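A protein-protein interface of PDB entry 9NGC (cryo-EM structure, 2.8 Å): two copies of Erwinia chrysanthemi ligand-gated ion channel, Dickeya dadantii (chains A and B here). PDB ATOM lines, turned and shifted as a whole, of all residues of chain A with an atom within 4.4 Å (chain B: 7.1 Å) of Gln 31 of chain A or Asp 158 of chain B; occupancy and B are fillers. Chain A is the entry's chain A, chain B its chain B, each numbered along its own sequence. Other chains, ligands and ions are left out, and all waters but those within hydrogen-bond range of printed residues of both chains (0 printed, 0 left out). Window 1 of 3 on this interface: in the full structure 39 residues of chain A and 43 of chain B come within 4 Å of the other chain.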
ATOM      1  N   ASN A  27       7.216   5.266  11.761  1.00  0.00           N
ATOM      2  CA  ASN A  27       8.610   5.554  11.447  1.00  0.00           C
ATOM      3  C   ASN A  27       9.209   4.308  10.806  1.00  0.00           C
ATOM      4  O   ASN A  27       9.584   3.361  11.500  1.00  0.00           O
ATOM      5  CB  ASN A  27       9.362   5.967  12.707  1.00  0.00           C
ATOM      6  CG  ASN A  27      10.797   6.346  12.433  1.00  0.00           C
ATOM      7  OD1 ASN A  27      11.110   6.927  11.396  1.00  0.00           O
ATOM      8  ND2 ASN A  27      11.677   6.040  13.373  1.00  0.00           N
ATOM      9  N   THR A  28       9.299   4.311   9.477  1.00  0.00           N
ATOM     10  CA  THR A  28       9.848   3.179   8.744  1.00  0.00           C
ATOM     11  C   THR A  28      11.365   3.099   8.827  1.00  0.00           C
ATOM     12  O   THR A  28      11.934   2.066   8.461  1.00  0.00           O
ATOM     13  CB  THR A  28       9.427   3.244   7.276  1.00  0.00           C
ATOM     14  OG1 THR A  28       9.652   4.565   6.772  1.00  0.00           O
ATOM     15  CG2 THR A  28       7.957   2.900   7.130  1.00  0.00           C
ATOM     16  N   LEU A  29      12.030   4.159   9.289  1.00  0.00           N
ATOM     17  CA  LEU A  29      13.473   4.101   9.477  1.00  0.00           C
ATOM     18  C   LEU A  29      13.832   3.196  10.646  1.00  0.00           C
ATOM     19  O   LEU A  29      14.853   2.501  10.602  1.00  0.00           O
ATOM     20  CB  LEU A  29      14.019   5.522   9.668  1.00  0.00           C
ATOM     21  CG  LEU A  29      15.510   5.879   9.614  1.00  0.00           C
ATOM     22  CD1 LEU A  29      15.636   7.364   9.341  1.00  0.00           C
ATOM     23  CD2 LEU A  29      16.278   5.541  10.886  1.00  0.00           C
ATOM     24  N   GLU A  30      13.011   3.190  11.695  1.00  0.00           N
ATOM     25  CA  GLU A  30      13.199   2.313  12.839  1.00  0.00           C
ATOM     26  C   GLU A  30      12.159   1.206  12.908  1.00  0.00           C
ATOM     27  O   GLU A  30      12.202   0.398  13.843  1.00  0.00           O
ATOM     28  CB  GLU A  30      13.170   3.130  14.133  1.00  0.00           C
ATOM     29  CG  GLU A  30      14.343   4.078  14.279  1.00  0.00           C
ATOM     30  CD  GLU A  30      14.280   4.888  15.555  1.00  0.00           C
ATOM     31  OE1 GLU A  30      13.256   4.800  16.265  1.00  0.00           O
ATOM     32  OE2 GLU A  30      15.251   5.618  15.844  1.00  0.00           O
ATOM     33  N   GLN A  31      11.236   1.155  11.941  1.00  0.00           N
ATOM     34  CA  GLN A  31      10.178   0.142  11.848  1.00  0.00           C
ATOM     35  C   GLN A  31       9.305   0.111  13.101  1.00  0.00           C
ATOM     36  O   GLN A  31       8.929  -0.954  13.592  1.00  0.00           O
ATOM     37  CB  GLN A  31      10.759  -1.240  11.542  1.00  0.00           C
ATOM     38  CG  GLN A  31      11.297  -1.358  10.131  1.00  0.00           C
ATOM     39  CD  GLN A  31      12.193  -2.558   9.943  1.00  0.00           C
ATOM     40  OE1 GLN A  31      11.865  -3.663  10.368  1.00  0.00           O
ATOM     41  NE2 GLN A  31      13.332  -2.348   9.299  1.00  0.00           N
ATOM     42  N   THR A  32       8.978   1.291  13.619  1.00  0.00           N
ATOM     43  CA  THR A  32       8.103   1.440  14.769  1.00  0.00           C
ATOM     44  C   THR A  32       6.896   2.292  14.402  1.00  0.00           C
ATOM     45  O   THR A  32       6.885   2.989  13.386  1.00  0.00           O
ATOM     46  CB  THR A  32       8.829   2.078  15.963  1.00  0.00           C
ATOM     47  OG1 THR A  32       9.172   3.431  15.652  1.00  0.00           O
ATOM     48  CG2 THR A  32      10.087   1.305  16.312  1.00  0.00           C
ATOM     49  N   SER A 111       6.493  -2.156  17.708  1.00  0.00           N
ATOM     50  CA  SER A 111       7.462  -2.490  16.676  1.00  0.00           C
ATOM     51  C   SER A 111       7.033  -3.749  15.939  1.00  0.00           C
ATOM     52  O   SER A 111       6.405  -4.640  16.514  1.00  0.00           O
ATOM     53  CB  SER A 111       8.864  -2.685  17.262  1.00  0.00           C
ATOM     54  OG  SER A 111       8.986  -3.957  17.871  1.00  0.00           O
ATOM     55  N   ASN A 112       7.388  -3.814  14.658  1.00  0.00           N
ATOM     56  CA  ASN A 112       7.091  -4.967  13.821  1.00  0.00           C
ATOM     57  C   ASN A 112       8.100  -5.019  12.685  1.00  0.00           C
ATOM     58  O   ASN A 112       8.640  -3.991  12.272  1.00  0.00           O
ATOM     59  CB  ASN A 112       5.663  -4.908  13.269  1.00  0.00           C
ATOM     60  CG  ASN A 112       5.193  -6.237  12.720  1.00  0.00           C
ATOM     61  OD1 ASN A 112       5.546  -7.295  13.234  1.00  0.00           O
ATOM     62  ND2 ASN A 112       4.390  -6.188  11.667  1.00  0.00           N
ATOM     63  N   ASP A 113       8.354  -6.227  12.187  1.00  0.00           N
ATOM     64  CA  ASP A 113       9.276  -6.401  11.072  1.00  0.00           C
ATOM     65  C   ASP A 113       8.620  -5.970   9.768  1.00  0.00           C
ATOM     66  O   ASP A 113       7.494  -6.370   9.463  1.00  0.00           O
ATOM     67  CB  ASP A 113       9.733  -7.854  10.976  1.00  0.00           C
ATOM     68  CG  ASP A 113      10.628  -8.259  12.126  1.00  0.00           C
ATOM     69  OD1 ASP A 113      11.334  -7.383  12.668  1.00  0.00           O
ATOM     70  OD2 ASP A 113      10.629  -9.454  12.489  1.00  0.00           O
ATOM     71  N   MET A 114       9.336  -5.164   8.992  1.00  0.00           N
ATOM     72  CA  MET A 114       8.827  -4.617   7.747  1.00  0.00           C
ATOM     73  C   MET A 114       9.701  -5.077   6.586  1.00  0.00           C
ATOM     74  O   MET A 114      10.911  -5.269   6.737  1.00  0.00           O
ATOM     75  CB  MET A 114       8.774  -3.092   7.811  1.00  0.00           C
ATOM     76  CG  MET A 114       7.751  -2.563   8.803  1.00  0.00           C
ATOM     77  SD  MET A 114       7.692  -0.767   8.889  1.00  0.00           S
ATOM     78  CE  MET A 114       6.486  -0.540  10.188  1.00  0.00           C
ATOM     79  N   PHE A 116      10.644  -4.193   2.788  1.00  0.00           N
ATOM     80  CA  PHE A 116      10.620  -3.160   1.752  1.00  0.00           C
ATOM     81  C   PHE A 116      11.272  -3.650   0.458  1.00  0.00           C
ATOM     82  O   PHE A 116      12.291  -3.123   0.025  1.00  0.00           O
ATOM     83  CB  PHE A 116      11.318  -1.900   2.251  1.00  0.00           C
ATOM     84  CG  PHE A 116      10.772  -1.353   3.537  1.00  0.00           C
ATOM     85  CD1 PHE A 116       9.542  -0.728   3.573  1.00  0.00           C
ATOM     86  CD2 PHE A 116      11.509  -1.433   4.706  1.00  0.00           C
ATOM     87  CE1 PHE A 116       9.044  -0.214   4.751  1.00  0.00           C
ATOM     88  CE2 PHE A 116      11.019  -0.917   5.885  1.00  0.00           C
ATOM     89  CZ  PHE A 116       9.786  -0.305   5.906  1.00  0.00           C
ATOM     90  N   ARG A 255      19.106   1.567   6.315  1.00  0.00           N
ATOM     91  CA  ARG A 255      20.192   1.110   5.452  1.00  0.00           C
ATOM     92  C   ARG A 255      19.997  -0.379   5.165  1.00  0.00           C
ATOM     93  O   ARG A 255      20.710  -1.251   5.663  1.00  0.00           O
ATOM     94  CB  ARG A 255      21.540   1.397   6.098  1.00  0.00           C
ATOM     95  CG  ARG A 255      21.879   2.872   6.168  1.00  0.00           C
ATOM     96  CD  ARG A 255      23.264   3.092   6.739  1.00  0.00           C
ATOM     97  NE  ARG A 255      23.290   4.210   7.673  1.00  0.00           N
ATOM     98  CZ  ARG A 255      23.501   4.089   8.975  1.00  0.00           C
ATOM     99  NH1 ARG A 255      23.716   2.910   9.534  1.00  0.00           N
ATOM    100  NH2 ARG A 255      23.493   5.179   9.736  1.00  0.00           N
ATOM    101  N   PRO A 257      19.732  -4.041   3.336  1.00  0.00           N
ATOM    102  CA  PRO A 257      20.699  -4.777   2.507  1.00  0.00           C
ATOM    103  C   PRO A 257      20.212  -5.078   1.099  1.00  0.00           C
ATOM    104  O   PRO A 257      20.963  -5.686   0.327  1.00  0.00           O
ATOM    105  CB  PRO A 257      20.917  -6.070   3.298  1.00  0.00           C
ATOM    106  CG  PRO A 257      19.646  -6.264   4.032  1.00  0.00           C
ATOM    107  CD  PRO A 257      19.146  -4.894   4.385  1.00  0.00           C
ATOM    108  N   ILE B  23      17.161  -7.117  20.354  1.00  0.00           N
ATOM    109  CA  ILE B  23      18.212  -6.109  20.317  1.00  0.00           C
ATOM    110  C   ILE B  23      17.897  -5.167  19.168  1.00  0.00           C
ATOM    111  O   ILE B  23      17.665  -5.613  18.040  1.00  0.00           O
ATOM    112  CB  ILE B  23      19.608  -6.738  20.150  1.00  0.00           C
ATOM    113  CG1 ILE B  23      19.978  -7.546  21.394  1.00  0.00           C
ATOM    114  CG2 ILE B  23      20.650  -5.666  19.890  1.00  0.00           C
ATOM    115  CD1 ILE B  23      21.411  -8.023  21.418  1.00  0.00           C
ATOM    116  N   TYR B  24      17.868  -3.871  19.456  1.00  0.00           N
ATOM    117  CA  TYR B  24      17.462  -2.882  18.472  1.00  0.00           C
ATOM    118  C   TYR B  24      18.181  -1.576  18.763  1.00  0.00           C
ATOM    119  O   TYR B  24      18.802  -1.407  19.813  1.00  0.00           O
ATOM    120  CB  TYR B  24      15.939  -2.694  18.469  1.00  0.00           C
ATOM    121  CG  TYR B  24      15.367  -2.216  19.784  1.00  0.00           C
ATOM    122  CD1 TYR B  24      15.067  -3.111  20.801  1.00  0.00           C
ATOM    123  CD2 TYR B  24      15.115  -0.871  20.004  1.00  0.00           C
ATOM    124  CE1 TYR B  24      14.549  -2.679  21.999  1.00  0.00           C
ATOM    125  CE2 TYR B  24      14.597  -0.431  21.198  1.00  0.00           C
ATOM    126  CZ  TYR B  24      14.314  -1.340  22.192  1.00  0.00           C
ATOM    127  OH  TYR B  24      13.794  -0.901  23.382  1.00  0.00           O
ATOM    128  N   GLY B  25      18.096  -0.652  17.814  1.00  0.00           N
ATOM    129  CA  GLY B  25      18.671   0.671  17.983  1.00  0.00           C
ATOM    130  C   GLY B  25      20.179   0.697  18.103  1.00  0.00           C
ATOM    131  O   GLY B  25      20.713   1.428  18.946  1.00  0.00           O
ATOM    132  N   VAL B  26      20.880  -0.078  17.277  1.00  0.00           N
ATOM    133  CA  VAL B  26      22.337  -0.132  17.331  1.00  0.00           C
ATOM    134  C   VAL B  26      22.895   1.144  16.722  1.00  0.00           C
ATOM    135  O   VAL B  26      22.969   1.282  15.497  1.00  0.00           O
ATOM    136  CB  VAL B  26      22.883  -1.374  16.607  1.00  0.00           C
ATOM    137  CG1 VAL B  26      24.378  -1.489  16.824  1.00  0.00           C
ATOM    138  CG2 VAL B  26      22.173  -2.624  17.090  1.00  0.00           C
ATOM    139  N   GLU B 156      18.454 -11.145  11.640  1.00  0.00           N
ATOM    140  CA  GLU B 156      19.178  -9.978  11.161  1.00  0.00           C
ATOM    141  C   GLU B 156      18.565  -8.718  11.758  1.00  0.00           C
ATOM    142  O   GLU B 156      17.517  -8.252  11.300  1.00  0.00           O
ATOM    143  CB  GLU B 156      19.165  -9.924   9.636  1.00  0.00           C
ATOM    144  CG  GLU B 156      20.020  -8.814   9.055  1.00  0.00           C
ATOM    145  CD  GLU B 156      20.019  -8.809   7.542  1.00  0.00           C
ATOM    146  OE1 GLU B 156      19.326  -9.657   6.942  1.00  0.00           O
ATOM    147  OE2 GLU B 156      20.716  -7.957   6.954  1.00  0.00           O
ATOM    148  N   ILE B 157      19.216  -8.181  12.787  1.00  0.00           N
ATOM    149  CA  ILE B 157      19.045  -6.778  13.137  1.00  0.00           C
ATOM    150  C   ILE B 157      19.545  -5.940  11.961  1.00  0.00           C
ATOM    151  O   ILE B 157      20.467  -6.344  11.250  1.00  0.00           O
ATOM    152  CB  ILE B 157      19.785  -6.445  14.458  1.00  0.00           C
ATOM    153  CG1 ILE B 157      19.211  -7.232  15.643  1.00  0.00           C
ATOM    154  CG2 ILE B 157      19.705  -4.971  14.847  1.00  0.00           C
ATOM    155  CD1 ILE B 157      19.859  -8.566  15.928  1.00  0.00           C
ATOM    156  N   ASP B 158      18.950  -4.750  11.783  1.00  0.00           N
ATOM    157  CA  ASP B 158      18.873  -3.972  10.543  1.00  0.00           C
ATOM    158  C   ASP B 158      20.095  -4.030   9.627  1.00  0.00           C
ATOM    159  O   ASP B 158      19.948  -4.056   8.400  1.00  0.00           O
ATOM    160  CB  ASP B 158      18.581  -2.510  10.887  1.00  0.00           C
ATOM    161  CG  ASP B 158      17.198  -2.317  11.480  1.00  0.00           C
ATOM    162  OD1 ASP B 158      16.206  -2.651  10.800  1.00  0.00           O
ATOM    163  OD2 ASP B 158      17.103  -1.825  12.622  1.00  0.00           O
ATOM    164  N   GLU B 159      21.304  -4.053  10.199  1.00  0.00           N
ATOM    165  CA  GLU B 159      22.481  -4.360   9.395  1.00  0.00           C
ATOM    166  C   GLU B 159      23.461  -5.284  10.117  1.00  0.00           C
ATOM    167  O   GLU B 159      24.633  -5.347   9.730  1.00  0.00           O
ATOM    168  CB  GLU B 159      23.186  -3.074   8.950  1.00  0.00           C
ATOM    169  CG  GLU B 159      23.787  -2.238  10.059  1.00  0.00           C
ATOM    170  CD  GLU B 159      24.403  -0.957   9.535  1.00  0.00           C
ATOM    171  OE1 GLU B 159      24.332  -0.723   8.311  1.00  0.00           O
ATOM    172  OE2 GLU B 159      24.961  -0.185  10.342  1.00  0.00           O
ATOM    173  N   TRP B 160      23.010  -6.022  11.130  1.00  0.00           N
ATOM    174  CA  TRP B 160      23.867  -6.902  11.914  1.00  0.00           C
ATOM    175  C   TRP B 160      23.319  -8.321  11.933  1.00  0.00           C
ATOM    176  O   TRP B 160      22.109  -8.532  12.027  1.00  0.00           O
ATOM    177  CB  TRP B 160      24.014  -6.393  13.349  1.00  0.00           C
ATOM    178  CG  TRP B 160      24.604  -5.032  13.442  1.00  0.00           C
ATOM    179  CD1 TRP B 160      23.934  -3.851  13.526  1.00  0.00           C
ATOM    180  CD2 TRP B 160      25.996  -4.707  13.471  1.00  0.00           C
ATOM    181  NE1 TRP B 160      24.822  -2.808  13.597  1.00  0.00           N
ATOM    182  CE2 TRP B 160      26.096  -3.309  13.568  1.00  0.00           C
ATOM    183  CE3 TRP B 160      27.168  -5.465  13.422  1.00  0.00           C
ATOM    184  CZ2 TRP B 160      27.319  -2.655  13.617  1.00  0.00           C
ATOM    185  CZ3 TRP B 160      28.379  -4.814  13.470  1.00  0.00           C
ATOM    186  CH2 TRP B 160      28.448  -3.423  13.567  1.00  0.00           C
ATOM    187  N   TRP B 161      24.224  -9.290  11.853  1.00  0.00           N
ATOM    188  CA  TRP B 161      23.902 -10.706  11.944  1.00  0.00           C
ATOM    189  C   TRP B 161      24.405 -11.257  13.267  1.00  0.00           C
ATOM    190  O   TRP B 161      25.567 -11.060  13.623  1.00  0.00           O
ATOM    191  CB  TRP B 161      24.550 -11.493  10.806  1.00  0.00           C
ATOM    192  CG  TRP B 161      23.828 -11.455   9.508  1.00  0.00           C
ATOM    193  CD1 TRP B 161      22.481 -11.411   9.315  1.00  0.00           C
ATOM    194  CD2 TRP B 161      24.419 -11.485   8.205  1.00  0.00           C
ATOM    195  NE1 TRP B 161      22.195 -11.402   7.972  1.00  0.00           N
ATOM    196  CE2 TRP B 161      23.370 -11.447   7.269  1.00  0.00           C
ATOM    197  CE3 TRP B 161      25.736 -11.535   7.740  1.00  0.00           C
ATOM    198  CZ2 TRP B 161      23.597 -11.458   5.896  1.00  0.00           C
ATOM    199  CZ3 TRP B 161      25.960 -11.546   6.379  1.00  0.00           C
ATOM    200  CH2 TRP B 161      24.897 -11.507   5.471  1.00  0.00           C
ATOM    201  N   ASN B 200      26.441  -6.690   7.957  1.00  0.00           N
ATOM    202  CA  ASN B 200      26.115  -7.040   6.583  1.00  0.00           C
ATOM    203  C   ASN B 200      26.671  -5.975   5.649  1.00  0.00           C
ATOM    204  O   ASN B 200      26.236  -4.819   5.720  1.00  0.00           O
ATOM    205  CB  ASN B 200      24.612  -7.153   6.404  1.00  0.00           C
ATOM    206  CG  ASN B 200      24.227  -8.028   5.230  1.00  0.00           C
ATOM    207  OD1 ASN B 200      25.072  -8.417   4.429  1.00  0.00           O
ATOM    208  ND2 ASN B 200      22.944  -8.335   5.119  1.00  0.00           N
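NE2 of Gln 31 of chain A lies within hydrogen-bond range of OD1 of Asp 158 of chain B, at 3.3 Å.
NH1 of Arg 255 of chain A lies within salt-bridge range of OE2 of Glu 159 of chain B, at 3.4 Å.
The side-chain carboxylate (OE2) of Glu 156 of chain B lies within hydrogen-bond range of the side-chain amide nitrogen (ND2) of Asn 200 of chain B, at 2.9 Å.
N of Asn 200 of chain B lies within hydrogen-bond range of O of Glu 159 of chain B (2.9 Å).
The backbone carbonyl oxygen of Gln 31 of chain A is in hydrogen-bond range of the backbone NH of Asn 112 of chain A.
The side-chain amide oxygen (OE1) of Gln 31 of chain A lies within hydrogen-bond range of the backbone NH (N) of Met 114 of chain A (3.2 Å).
Among the printed residues, pairs that only touch across the chains: Arg 255 of chain A with Asp 158 of chain B (3.99 Å), Pro 257 of chain A with Glu 156 of chain B (3.5 Å) and Pro 257 of chain A with Asn 200 of chain B (3.5 Å).
Of the printed residues of chain B, Pro 257 of chain A touches Glu 156 and Asn 200.
Of the printed residues of chain A, Glu 156 of chain B touches Pro 257 (3.5 Å).
Printed residues of chain A within 4 Å of Asp 158 of chain B: Gln 31 (3.3 Å) and Arg 255 (3.99 Å).
The nearest printed residue of chain B that does not touch Gln 31 of chain A is Glu 156 of chain B (7.3 Å).
The nearest printed residue of chain A that does not touch Asp 158 of chain B is Pro 257 of chain A (4.2 Å).
The nearest printed residue of chain B that does not touch Arg 255 of chain A is Val 26 of chain B (6.2 Å).
Hydrophobic or aromatic side chains of chain A that line the printed part of chain B: Pro 257.
Of the 11 printed residues of chain B, 4 touch a printed residue of chain A.
Among the printed residues, 5 pairs touch across the chains.
Among the printed residues, Asp or Glu carboxylates within 4 Å of a Lys or Arg side-chain nitrogen of the other chain: Arg 255 of chain A with Glu 159 of chain B (3.4 Å).
No position is printed for both chains.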
